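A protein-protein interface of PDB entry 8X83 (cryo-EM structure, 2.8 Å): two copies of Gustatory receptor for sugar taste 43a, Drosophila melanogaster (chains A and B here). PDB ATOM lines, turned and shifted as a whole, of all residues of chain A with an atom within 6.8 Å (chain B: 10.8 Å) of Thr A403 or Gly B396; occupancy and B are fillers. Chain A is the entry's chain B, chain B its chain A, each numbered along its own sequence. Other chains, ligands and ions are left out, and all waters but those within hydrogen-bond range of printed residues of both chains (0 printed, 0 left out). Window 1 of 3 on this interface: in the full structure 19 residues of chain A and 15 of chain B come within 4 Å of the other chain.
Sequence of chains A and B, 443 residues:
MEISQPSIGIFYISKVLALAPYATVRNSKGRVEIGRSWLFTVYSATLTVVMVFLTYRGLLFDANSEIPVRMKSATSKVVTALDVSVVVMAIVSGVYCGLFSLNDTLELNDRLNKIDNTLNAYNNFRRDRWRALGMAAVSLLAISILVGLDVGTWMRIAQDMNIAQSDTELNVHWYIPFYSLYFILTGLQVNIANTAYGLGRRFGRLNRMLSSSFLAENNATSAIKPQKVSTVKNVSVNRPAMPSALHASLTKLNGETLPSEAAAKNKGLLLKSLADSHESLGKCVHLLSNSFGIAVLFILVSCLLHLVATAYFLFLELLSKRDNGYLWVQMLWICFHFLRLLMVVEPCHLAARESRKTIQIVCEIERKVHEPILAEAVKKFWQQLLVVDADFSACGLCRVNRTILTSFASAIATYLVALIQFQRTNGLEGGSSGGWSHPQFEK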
ATOM      1  N   VAL A 345      17.420  -7.257 -12.182  1.00  0.00           N
ATOM      2  CA  VAL A 345      17.764  -7.174 -10.765  1.00  0.00           C
ATOM      3  C   VAL A 345      18.745  -8.262 -10.329  1.00  0.00           C
ATOM      4  O   VAL A 345      19.742  -7.962  -9.665  1.00  0.00           O
ATOM      5  CB  VAL A 345      16.475  -7.230  -9.926  1.00  0.00           C
ATOM      6  CG1 VAL A 345      16.769  -7.679  -8.505  1.00  0.00           C
ATOM      7  CG2 VAL A 345      15.784  -5.883  -9.928  1.00  0.00           C
ATOM      8  N   HIS A 349      22.527  -8.294  -8.161  1.00  0.00           N
ATOM      9  CA  HIS A 349      22.515  -8.927  -6.848  1.00  0.00           C
ATOM     10  C   HIS A 349      23.538 -10.051  -6.775  1.00  0.00           C
ATOM     11  O   HIS A 349      24.283 -10.161  -5.797  1.00  0.00           O
ATOM     12  CB  HIS A 349      21.114  -9.451  -6.540  1.00  0.00           C
ATOM     13  CG  HIS A 349      20.986 -10.075  -5.186  1.00  0.00           C
ATOM     14  ND1 HIS A 349      20.645  -9.351  -4.065  1.00  0.00           N
ATOM     15  CD2 HIS A 349      21.148 -11.355  -4.774  1.00  0.00           C
ATOM     16  CE1 HIS A 349      20.606 -10.157  -3.019  1.00  0.00           C
ATOM     17  NE2 HIS A 349      20.907 -11.378  -3.422  1.00  0.00           N
ATOM     18  N   ARG A 399      20.299   1.357  -5.396  1.00  0.00           N
ATOM     19  CA  ARG A 399      21.198   0.230  -5.593  1.00  0.00           C
ATOM     20  C   ARG A 399      20.375  -0.965  -6.056  1.00  0.00           C
ATOM     21  O   ARG A 399      19.446  -1.392  -5.365  1.00  0.00           O
ATOM     22  CB  ARG A 399      21.948  -0.108  -4.303  1.00  0.00           C
ATOM     23  CG  ARG A 399      23.101   0.834  -3.917  1.00  0.00           C
ATOM     24  CD  ARG A 399      24.063   1.169  -5.058  1.00  0.00           C
ATOM     25  NE  ARG A 399      24.886   2.332  -4.745  1.00  0.00           N
ATOM     26  CZ  ARG A 399      26.206   2.391  -4.873  1.00  0.00           C
ATOM     27  NH1 ARG A 399      26.908   1.365  -5.328  1.00  0.00           N
ATOM     28  NH2 ARG A 399      26.840   3.512  -4.541  1.00  0.00           N
ATOM     29  N   VAL A 400      20.715  -1.495  -7.228  1.00  0.00           N
ATOM     30  CA  VAL A 400      19.920  -2.536  -7.872  1.00  0.00           C
ATOM     31  C   VAL A 400      20.259  -3.861  -7.198  1.00  0.00           C
ATOM     32  O   VAL A 400      21.358  -4.394  -7.353  1.00  0.00           O
ATOM     33  CB  VAL A 400      20.164  -2.586  -9.379  1.00  0.00           C
ATOM     34  CG1 VAL A 400      19.164  -3.511 -10.045  1.00  0.00           C
ATOM     35  CG2 VAL A 400      20.069  -1.196  -9.973  1.00  0.00           C
ATOM     36  N   ASN A 401      19.301  -4.391  -6.444  1.00  0.00           N
ATOM     37  CA  ASN A 401      19.418  -5.693  -5.808  1.00  0.00           C
ATOM     38  C   ASN A 401      18.006  -6.237  -5.614  1.00  0.00           C
ATOM     39  O   ASN A 401      17.030  -5.668  -6.111  1.00  0.00           O
ATOM     40  CB  ASN A 401      20.200  -5.591  -4.491  1.00  0.00           C
ATOM     41  CG  ASN A 401      19.841  -4.359  -3.693  1.00  0.00           C
ATOM     42  OD1 ASN A 401      18.676  -3.978  -3.605  1.00  0.00           O
ATOM     43  ND2 ASN A 401      20.843  -3.734  -3.093  1.00  0.00           N
ATOM     44  N   ARG A 402      17.893  -7.348  -4.889  1.00  0.00           N
ATOM     45  CA  ARG A 402      16.590  -7.963  -4.682  1.00  0.00           C
ATOM     46  C   ARG A 402      15.701  -7.144  -3.758  1.00  0.00           C
ATOM     47  O   ARG A 402      14.473  -7.233  -3.863  1.00  0.00           O
ATOM     48  CB  ARG A 402      16.763  -9.376  -4.131  1.00  0.00           C
ATOM     49  CG  ARG A 402      16.879 -10.430  -5.211  1.00  0.00           C
ATOM     50  CD  ARG A 402      17.093 -11.810  -4.632  1.00  0.00           C
ATOM     51  NE  ARG A 402      17.698 -12.712  -5.603  1.00  0.00           N
ATOM     52  CZ  ARG A 402      18.074 -13.954  -5.338  1.00  0.00           C
ATOM     53  NH1 ARG A 402      17.923 -14.479  -4.134  1.00  0.00           N
ATOM     54  NH2 ARG A 402      18.617 -14.687  -6.304  1.00  0.00           N
ATOM     55  N   THR A 403      16.286  -6.340  -2.867  1.00  0.00           N
ATOM     56  CA  THR A 403      15.484  -5.480  -2.006  1.00  0.00           C
ATOM     57  C   THR A 403      14.534  -4.604  -2.808  1.00  0.00           C
ATOM     58  O   THR A 403      13.383  -4.421  -2.397  1.00  0.00           O
ATOM     59  CB  THR A 403      16.384  -4.597  -1.142  1.00  0.00           C
ATOM     60  OG1 THR A 403      17.070  -3.652  -1.971  1.00  0.00           O
ATOM     61  CG2 THR A 403      17.399  -5.436  -0.381  1.00  0.00           C
ATOM     62  N   ILE A 404      14.993  -4.064  -3.939  1.00  0.00           N
ATOM     63  CA  ILE A 404      14.120  -3.302  -4.826  1.00  0.00           C
ATOM     64  C   ILE A 404      12.785  -4.006  -5.000  1.00  0.00           C
ATOM     65  O   ILE A 404      11.723  -3.383  -4.863  1.00  0.00           O
ATOM     66  CB  ILE A 404      14.823  -3.070  -6.180  1.00  0.00           C
ATOM     67  CG1 ILE A 404      15.691  -1.811  -6.105  1.00  0.00           C
ATOM     68  CG2 ILE A 404      13.804  -3.002  -7.323  1.00  0.00           C
ATOM     69  CD1 ILE A 404      16.299  -1.395  -7.419  1.00  0.00           C
ATOM     70  N   LEU A 405      12.811  -5.309  -5.295  1.00  0.00           N
ATOM     71  CA  LEU A 405      11.570  -6.052  -5.481  1.00  0.00           C
ATOM     72  C   LEU A 405      10.582  -5.748  -4.366  1.00  0.00           C
ATOM     73  O   LEU A 405       9.454  -5.309  -4.626  1.00  0.00           O
ATOM     74  CB  LEU A 405      11.863  -7.549  -5.542  1.00  0.00           C
ATOM     75  CG  LEU A 405      12.784  -8.014  -6.670  1.00  0.00           C
ATOM     76  CD1 LEU A 405      13.042  -9.504  -6.560  1.00  0.00           C
ATOM     77  CD2 LEU A 405      12.195  -7.673  -8.024  1.00  0.00           C
ATOM     78  N   THR A 406      10.999  -5.946  -3.113  1.00  0.00           N
ATOM     79  CA  THR A 406      10.129  -5.627  -1.987  1.00  0.00           C
ATOM     80  C   THR A 406       9.536  -4.233  -2.139  1.00  0.00           C
ATOM     81  O   THR A 406       8.311  -4.071  -2.179  1.00  0.00           O
ATOM     82  CB  THR A 406      10.909  -5.734  -0.676  1.00  0.00           C
ATOM     83  OG1 THR A 406      11.490  -7.039  -0.568  1.00  0.00           O
ATOM     84  CG2 THR A 406       9.995  -5.495   0.510  1.00  0.00           C
ATOM     85  N   SER A 407      10.395  -3.218  -2.260  1.00  0.00           N
ATOM     86  CA  SER A 407       9.902  -1.860  -2.457  1.00  0.00           C
ATOM     87  C   SER A 407       8.910  -1.807  -3.607  1.00  0.00           C
ATOM     88  O   SER A 407       7.799  -1.284  -3.456  1.00  0.00           O
ATOM     89  CB  SER A 407      11.073  -0.913  -2.713  1.00  0.00           C
ATOM     90  OG  SER A 407      12.005  -0.958  -1.649  1.00  0.00           O
ATOM     91  N   PHE A 408       9.279  -2.380  -4.755  1.00  0.00           N
ATOM     92  CA  PHE A 408       8.365  -2.401  -5.890  1.00  0.00           C
ATOM     93  C   PHE A 408       7.004  -2.934  -5.471  1.00  0.00           C
ATOM     94  O   PHE A 408       5.974  -2.290  -5.713  1.00  0.00           O
ATOM     95  CB  PHE A 408       8.948  -3.252  -7.016  1.00  0.00           C
ATOM     96  CG  PHE A 408       9.643  -2.458  -8.082  1.00  0.00           C
ATOM     97  CD1 PHE A 408      10.513  -1.434  -7.750  1.00  0.00           C
ATOM     98  CD2 PHE A 408       9.430  -2.739  -9.418  1.00  0.00           C
ATOM     99  CE1 PHE A 408      11.153  -0.707  -8.730  1.00  0.00           C
ATOM    100  CE2 PHE A 408      10.069  -2.016 -10.402  1.00  0.00           C
ATOM    101  CZ  PHE A 408      10.930  -0.998 -10.058  1.00  0.00           C
ATOM    102  N   HIS B 286      23.967 -18.825   7.662  1.00  0.00           N
ATOM    103  CA  HIS B 286      23.884 -18.673   6.214  1.00  0.00           C
ATOM    104  C   HIS B 286      23.305 -19.916   5.547  1.00  0.00           C
ATOM    105  O   HIS B 286      22.611 -19.805   4.534  1.00  0.00           O
ATOM    106  CB  HIS B 286      25.261 -18.350   5.639  1.00  0.00           C
ATOM    107  CG  HIS B 286      25.750 -16.981   5.991  1.00  0.00           C
ATOM    108  ND1 HIS B 286      25.023 -15.842   5.722  1.00  0.00           N
ATOM    109  CD2 HIS B 286      26.891 -16.566   6.589  1.00  0.00           C
ATOM    110  CE1 HIS B 286      25.694 -14.784   6.141  1.00  0.00           C
ATOM    111  NE2 HIS B 286      26.831 -15.197   6.672  1.00  0.00           N
ATOM    112  N   LEU B 288      21.047 -22.016   7.002  1.00  0.00           N
ATOM    113  CA  LEU B 288      19.620 -21.925   7.283  1.00  0.00           C
ATOM    114  C   LEU B 288      18.953 -20.928   6.349  1.00  0.00           C
ATOM    115  O   LEU B 288      17.852 -21.176   5.847  1.00  0.00           O
ATOM    116  CB  LEU B 288      19.403 -21.534   8.743  1.00  0.00           C
ATOM    117  CG  LEU B 288      17.986 -21.159   9.181  1.00  0.00           C
ATOM    118  CD1 LEU B 288      17.077 -22.372   9.198  1.00  0.00           C
ATOM    119  CD2 LEU B 288      18.029 -20.503  10.546  1.00  0.00           C
ATOM    120  N   SER B 289      19.605 -19.789   6.104  1.00  0.00           N
ATOM    121  CA  SER B 289      19.077 -18.834   5.139  1.00  0.00           C
ATOM    122  C   SER B 289      18.977 -19.445   3.747  1.00  0.00           C
ATOM    123  O   SER B 289      17.884 -19.512   3.185  1.00  0.00           O
ATOM    124  CB  SER B 289      19.945 -17.580   5.101  1.00  0.00           C
ATOM    125  OG  SER B 289      20.344 -17.198   6.405  1.00  0.00           O
ATOM    126  N   ASN B 290      20.086 -19.934   3.194  1.00  0.00           N
ATOM    127  CA  ASN B 290      20.059 -20.469   1.839  1.00  0.00           C
ATOM    128  C   ASN B 290      19.060 -21.612   1.702  1.00  0.00           C
ATOM    129  O   ASN B 290      18.608 -21.904   0.589  1.00  0.00           O
ATOM    130  CB  ASN B 290      21.458 -20.933   1.437  1.00  0.00           C
ATOM    131  CG  ASN B 290      21.454 -21.801   0.197  1.00  0.00           C
ATOM    132  OD1 ASN B 290      21.246 -21.313  -0.914  1.00  0.00           O
ATOM    133  ND2 ASN B 290      21.689 -23.094   0.379  1.00  0.00           N
ATOM    134  N   SER B 291      18.697 -22.261   2.810  1.00  0.00           N
ATOM    135  CA  SER B 291      17.793 -23.402   2.726  1.00  0.00           C
ATOM    136  C   SER B 291      16.330 -22.994   2.875  1.00  0.00           C
ATOM    137  O   SER B 291      15.473 -23.500   2.143  1.00  0.00           O
ATOM    138  CB  SER B 291      18.163 -24.439   3.784  1.00  0.00           C
ATOM    139  OG  SER B 291      19.208 -25.276   3.327  1.00  0.00           O
ATOM    140  N   PHE B 292      16.015 -22.091   3.809  1.00  0.00           N
ATOM    141  CA  PHE B 292      14.630 -21.778   4.144  1.00  0.00           C
ATOM    142  C   PHE B 292      14.312 -20.289   4.036  1.00  0.00           C
ATOM    143  O   PHE B 292      13.365 -19.818   4.670  1.00  0.00           O
ATOM    144  CB  PHE B 292      14.306 -22.276   5.554  1.00  0.00           C
ATOM    145  CG  PHE B 292      14.309 -23.769   5.682  1.00  0.00           C
ATOM    146  CD1 PHE B 292      15.485 -24.451   5.933  1.00  0.00           C
ATOM    147  CD2 PHE B 292      13.138 -24.493   5.551  1.00  0.00           C
ATOM    148  CE1 PHE B 292      15.493 -25.824   6.050  1.00  0.00           C
ATOM    149  CE2 PHE B 292      13.141 -25.866   5.667  1.00  0.00           C
ATOM    150  CZ  PHE B 292      14.320 -26.532   5.917  1.00  0.00           C
ATOM    151  N   GLY B 293      15.064 -19.536   3.231  1.00  0.00           N
ATOM    152  CA  GLY B 293      14.763 -18.127   3.069  1.00  0.00           C
ATOM    153  C   GLY B 293      13.476 -17.878   2.318  1.00  0.00           C
ATOM    154  O   GLY B 293      12.714 -16.978   2.673  1.00  0.00           O
ATOM    155  N   ILE B 294      13.213 -18.665   1.276  1.00  0.00           N
ATOM    156  CA  ILE B 294      11.949 -18.540   0.562  1.00  0.00           C
ATOM    157  C   ILE B 294      10.790 -18.902   1.485  1.00  0.00           C
ATOM    158  O   ILE B 294       9.732 -18.258   1.464  1.00  0.00           O
ATOM    159  CB  ILE B 294      11.979 -19.411  -0.709  1.00  0.00           C
ATOM    160  CG1 ILE B 294      10.740 -19.164  -1.566  1.00  0.00           C
ATOM    161  CG2 ILE B 294      12.087 -20.884  -0.356  1.00  0.00           C
ATOM    162  CD1 ILE B 294      10.816 -17.900  -2.395  1.00  0.00           C
ATOM    163  N   ALA B 295      10.980 -19.922   2.324  1.00  0.00           N
ATOM    164  CA  ALA B 295       9.952 -20.292   3.289  1.00  0.00           C
ATOM    165  C   ALA B 295       9.698 -19.166   4.282  1.00  0.00           C
ATOM    166  O   ALA B 295       8.543 -18.851   4.589  1.00  0.00           O
ATOM    167  CB  ALA B 295      10.359 -21.566   4.024  1.00  0.00           C
ATOM    168  N   VAL B 296      10.762 -18.551   4.799  1.00  0.00           N
ATOM    169  CA  VAL B 296      10.598 -17.453   5.747  1.00  0.00           C
ATOM    170  C   VAL B 296       9.928 -16.262   5.074  1.00  0.00           C
ATOM    171  O   VAL B 296       9.090 -15.580   5.676  1.00  0.00           O
ATOM    172  CB  VAL B 296      11.959 -17.067   6.355  1.00  0.00           C
ATOM    173  CG1 VAL B 296      11.864 -15.732   7.073  1.00  0.00           C
ATOM    174  CG2 VAL B 296      12.442 -18.149   7.297  1.00  0.00           C
ATOM    175  N   LEU B 297      10.289 -15.992   3.820  1.00  0.00           N
ATOM    176  CA  LEU B 297       9.681 -14.882   3.096  1.00  0.00           C
ATOM    177  C   LEU B 297       8.188 -15.102   2.910  1.00  0.00           C
ATOM    178  O   LEU B 297       7.384 -14.186   3.125  1.00  0.00           O
ATOM    179  CB  LEU B 297      10.371 -14.711   1.745  1.00  0.00           C
ATOM    180  CG  LEU B 297       9.868 -13.580   0.848  1.00  0.00           C
ATOM    181  CD1 LEU B 297      10.483 -12.259   1.272  1.00  0.00           C
ATOM    182  CD2 LEU B 297      10.189 -13.887  -0.599  1.00  0.00           C
ATOM    183  N   PHE B 298       7.794 -16.310   2.509  1.00  0.00           N
ATOM    184  CA  PHE B 298       6.374 -16.586   2.352  1.00  0.00           C
ATOM    185  C   PHE B 298       5.654 -16.623   3.691  1.00  0.00           C
ATOM    186  O   PHE B 298       4.481 -16.251   3.763  1.00  0.00           O
ATOM    187  CB  PHE B 298       6.164 -17.896   1.593  1.00  0.00           C
ATOM    188  CG  PHE B 298       6.411 -17.780   0.119  1.00  0.00           C
ATOM    189  CD1 PHE B 298       5.706 -16.866  -0.642  1.00  0.00           C
ATOM    190  CD2 PHE B 298       7.333 -18.591  -0.512  1.00  0.00           C
ATOM    191  CE1 PHE B 298       5.930 -16.751  -1.994  1.00  0.00           C
ATOM    192  CE2 PHE B 298       7.553 -18.482  -1.871  1.00  0.00           C
ATOM    193  CZ  PHE B 298       6.850 -17.562  -2.611  1.00  0.00           C
ATOM    194  N   LEU B 300       6.411 -14.614   6.180  1.00  0.00           N
ATOM    195  CA  LEU B 300       6.213 -13.202   6.488  1.00  0.00           C
ATOM    196  C   LEU B 300       5.080 -12.611   5.658  1.00  0.00           C
ATOM    197  O   LEU B 300       4.247 -11.854   6.177  1.00  0.00           O
ATOM    198  CB  LEU B 300       7.508 -12.431   6.247  1.00  0.00           C
ATOM    199  CG  LEU B 300       8.676 -12.777   7.169  1.00  0.00           C
ATOM    200  CD1 LEU B 300       9.958 -12.165   6.642  1.00  0.00           C
ATOM    201  CD2 LEU B 300       8.405 -12.314   8.587  1.00  0.00           C
ATOM    202  N   ASP B 389      29.055 -11.385   8.581  1.00  0.00           N
ATOM    203  CA  ASP B 389      27.696 -11.152   8.094  1.00  0.00           C
ATOM    204  C   ASP B 389      26.753 -11.999   8.940  1.00  0.00           C
ATOM    205  O   ASP B 389      26.662 -13.216   8.765  1.00  0.00           O
ATOM    206  CB  ASP B 389      27.588 -11.489   6.612  1.00  0.00           C
ATOM    207  CG  ASP B 389      26.231 -11.140   6.032  1.00  0.00           C
ATOM    208  OD1 ASP B 389      25.889 -11.667   4.952  1.00  0.00           O
ATOM    209  OD2 ASP B 389      25.504 -10.345   6.662  1.00  0.00           O
ATOM    210  N   ASP B 391      23.256 -10.943   9.980  1.00  0.00           N
ATOM    211  CA  ASP B 391      21.820 -10.802   9.786  1.00  0.00           C
ATOM    212  C   ASP B 391      21.288 -11.885   8.855  1.00  0.00           C
ATOM    213  O   ASP B 391      21.937 -12.268   7.879  1.00  0.00           O
ATOM    214  CB  ASP B 391      21.498  -9.415   9.227  1.00  0.00           C
ATOM    215  CG  ASP B 391      20.439  -8.683  10.038  1.00  0.00           C
ATOM    216  OD1 ASP B 391      20.288  -7.460   9.841  1.00  0.00           O
ATOM    217  OD2 ASP B 391      19.750  -9.326  10.859  1.00  0.00           O
ATOM    218  N   PHE B 392      20.092 -12.378   9.171  1.00  0.00           N
ATOM    219  CA  PHE B 392      19.451 -13.422   8.388  1.00  0.00           C
ATOM    220  C   PHE B 392      18.754 -12.802   7.184  1.00  0.00           C
ATOM    221  O   PHE B 392      18.015 -11.824   7.321  1.00  0.00           O
ATOM    222  CB  PHE B 392      18.449 -14.182   9.259  1.00  0.00           C
ATOM    223  CG  PHE B 392      17.706 -15.272   8.541  1.00  0.00           C
ATOM    224  CD1 PHE B 392      16.660 -14.979   7.682  1.00  0.00           C
ATOM    225  CD2 PHE B 392      18.040 -16.598   8.744  1.00  0.00           C
ATOM    226  CE1 PHE B 392      15.977 -15.984   7.030  1.00  0.00           C
ATOM    227  CE2 PHE B 392      17.360 -17.604   8.097  1.00  0.00           C
ATOM    228  CZ  PHE B 392      16.327 -17.297   7.239  1.00  0.00           C
ATOM    229  N   SER B 393      18.985 -13.376   6.007  1.00  0.00           N
ATOM    230  CA  SER B 393      18.439 -12.864   4.757  1.00  0.00           C
ATOM    231  C   SER B 393      17.364 -13.810   4.243  1.00  0.00           C
ATOM    232  O   SER B 393      17.598 -15.018   4.127  1.00  0.00           O
ATOM    233  CB  SER B 393      19.539 -12.699   3.709  1.00  0.00           C
ATOM    234  OG  SER B 393      19.044 -12.051   2.551  1.00  0.00           O
ATOM    235  N   ALA B 394      16.191 -13.256   3.932  1.00  0.00           N
ATOM    236  CA  ALA B 394      15.083 -14.034   3.379  1.00  0.00           C
ATOM    237  C   ALA B 394      15.141 -13.935   1.857  1.00  0.00           C
ATOM    238  O   ALA B 394      14.423 -13.162   1.220  1.00  0.00           O
ATOM    239  CB  ALA B 394      13.753 -13.539   3.927  1.00  0.00           C
ATOM    240  N   CYS B 395      16.021 -14.744   1.271  1.00  0.00           N
ATOM    241  CA  CYS B 395      16.240 -14.791  -0.171  1.00  0.00           C
ATOM    242  C   CYS B 395      16.718 -13.458  -0.730  1.00  0.00           C
ATOM    243  O   CYS B 395      16.499 -13.164  -1.909  1.00  0.00           O
ATOM    244  CB  CYS B 395      14.972 -15.242  -0.905  1.00  0.00           C
ATOM    245  SG  CYS B 395      14.600 -16.997  -0.719  1.00  0.00           S
ATOM    246  N   GLY B 396      17.372 -12.642   0.094  1.00  0.00           N
ATOM    247  CA  GLY B 396      17.858 -11.349  -0.332  1.00  0.00           C
ATOM    248  C   GLY B 396      16.815 -10.260  -0.385  1.00  0.00           C
ATOM    249  O   GLY B 396      17.172  -9.096  -0.599  1.00  0.00           O
ATOM    250  N   LEU B 397      15.538 -10.592  -0.194  1.00  0.00           N
ATOM    251  CA  LEU B 397      14.488  -9.585  -0.239  1.00  0.00           C
ATOM    252  C   LEU B 397      14.541  -8.669   0.975  1.00  0.00           C
ATOM    253  O   LEU B 397      14.316  -7.459   0.854  1.00  0.00           O
ATOM    254  CB  LEU B 397      13.120 -10.262  -0.331  1.00  0.00           C
ATOM    255  CG  LEU B 397      12.663 -10.728  -1.714  1.00  0.00           C
ATOM    256  CD1 LEU B 397      12.405  -9.542  -2.614  1.00  0.00           C
ATOM    257  CD2 LEU B 397      13.681 -11.655  -2.346  1.00  0.00           C
ATOM    258  N   CYS B 398      14.834  -9.224   2.148  1.00  0.00           N
ATOM    259  CA  CYS B 398      14.863  -8.442   3.373  1.00  0.00           C
ATOM    260  C   CYS B 398      15.730  -9.159   4.395  1.00  0.00           C
ATOM    261  O   CYS B 398      15.947 -10.370   4.314  1.00  0.00           O
ATOM    262  CB  CYS B 398      13.454  -8.227   3.931  1.00  0.00           C
ATOM    263  SG  CYS B 398      12.688  -9.729   4.578  1.00  0.00           S
ATOM    264  N   ARG B 399      16.222  -8.388   5.360  1.00  0.00           N
ATOM    265  CA  ARG B 399      16.931  -8.941   6.504  1.00  0.00           C
ATOM    266  C   ARG B 399      15.943  -9.097   7.652  1.00  0.00           C
ATOM    267  O   ARG B 399      15.321  -8.121   8.081  1.00  0.00           O
ATOM    268  CB  ARG B 399      18.092  -8.037   6.920  1.00  0.00           C
ATOM    269  CG  ARG B 399      19.346  -8.083   6.031  1.00  0.00           C
ATOM    270  CD  ARG B 399      19.827  -9.491   5.675  1.00  0.00           C
ATOM    271  NE  ARG B 399      20.758  -9.474   4.551  1.00  0.00           N
ATOM    272  CZ  ARG B 399      21.936 -10.086   4.527  1.00  0.00           C
ATOM    273  NH1 ARG B 399      22.372 -10.801   5.552  1.00  0.00           N
ATOM    274  NH2 ARG B 399      22.696  -9.983   3.441  1.00  0.00           N
ATOM    275  N   VAL B 400      15.797 -10.326   8.140  1.00  0.00           N
ATOM    276  CA  VAL B 400      14.774 -10.655   9.128  1.00  0.00           C
ATOM    277  C   VAL B 400      15.282 -10.197  10.491  1.00  0.00           C
ATOM    278  O   VAL B 400      16.219 -10.768  11.049  1.00  0.00           O
ATOM    279  CB  VAL B 400      14.436 -12.145   9.119  1.00  0.00           C
ATOM    280  CG1 VAL B 400      13.220 -12.415   9.984  1.00  0.00           C
ATOM    281  CG2 VAL B 400      14.187 -12.618   7.702  1.00  0.00           C
ATOM    282  N   ILE B 404      11.609  -5.210  10.679  1.00  0.00           N
ATOM    283  CA  ILE B 404      10.503  -5.682   9.853  1.00  0.00           C
ATOM    284  C   ILE B 404       9.169  -5.364  10.509  1.00  0.00           C
ATOM    285  O   ILE B 404       8.264  -4.821   9.861  1.00  0.00           O
ATOM    286  CB  ILE B 404      10.659  -7.194   9.583  1.00  0.00           C
ATOM    287  CG1 ILE B 404      11.546  -7.412   8.355  1.00  0.00           C
ATOM    288  CG2 ILE B 404       9.291  -7.869   9.434  1.00  0.00           C
ATOM    289  CD1 ILE B 404      11.638  -8.846   7.900  1.00  0.00           C
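O of Cys B395 sits at hydrogen-bond distance from NH1 of Arg A402.
The side-chain hydroxyl (OG1) of Thr A406 lies within hydrogen-bond range of the backbone carbonyl oxygen (O) of Leu B397, 3.2 Å away.
The backbone NH (N) of Ile B294 sits at hydrogen-bond distance from the side-chain sulfur (SG) of Cys B395.
N of Gly B396 sits at hydrogen-bond distance from OG of Ser B393.
The backbone NH of Thr A403 sits close to the side-chain amide oxygen of Asn A401 (3.4 Å).
Among the printed residues, pairs that only touch across the chains: Arg A402 with Gly B396, Arg A402 with Leu B397, Thr A403 with Gly B396, Thr A403 with Leu B397 and Leu A405 with Leu B397.
No residue of chain B comes within 4 Å of Asn A401.
Printed residues of chain B within 4 Å of Thr A403: Gly B396 and Leu B397.
No residue of chain B comes within 4 Å of Ile A404.
Leu A405 touches just one residue of chain B: Leu B397.
No residue of chain B comes within 4 Å of Ser A407.
Printed residues of chain A within 4 Å of Cys B395: Arg A402 (3.0 Å).
Gly B396 touches two residues of chain A.
Of the printed residues of chain A, Leu B397 touches Arg A402 (3.3 Å), Thr A403 (3.7 Å), Leu A405 (3.6 Å) and Thr A406 (3.2 Å).
The nearest residue of chain A that does not touch Gly B396 is His A349 (4.02 Å).
Of the 25 printed residues of chain B, 3 touch a printed residue of chain A.
Hydrophobic or aromatic side chains of chain B within 4 Å of the printed part of chain A: Leu B397.
Of the 12 printed residues of chain A, 4 touch a printed residue of chain B.
Among the printed residues, no Asp or Glu carboxylate lies within 4 Å of a Lys or Arg side-chain nitrogen of the other chain.
Positions printed for both chains: 399, 400 and 404.
Of the 7 pairs that touch across the chains among the printed residues, none has its exchanged pair printed and touching as well.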
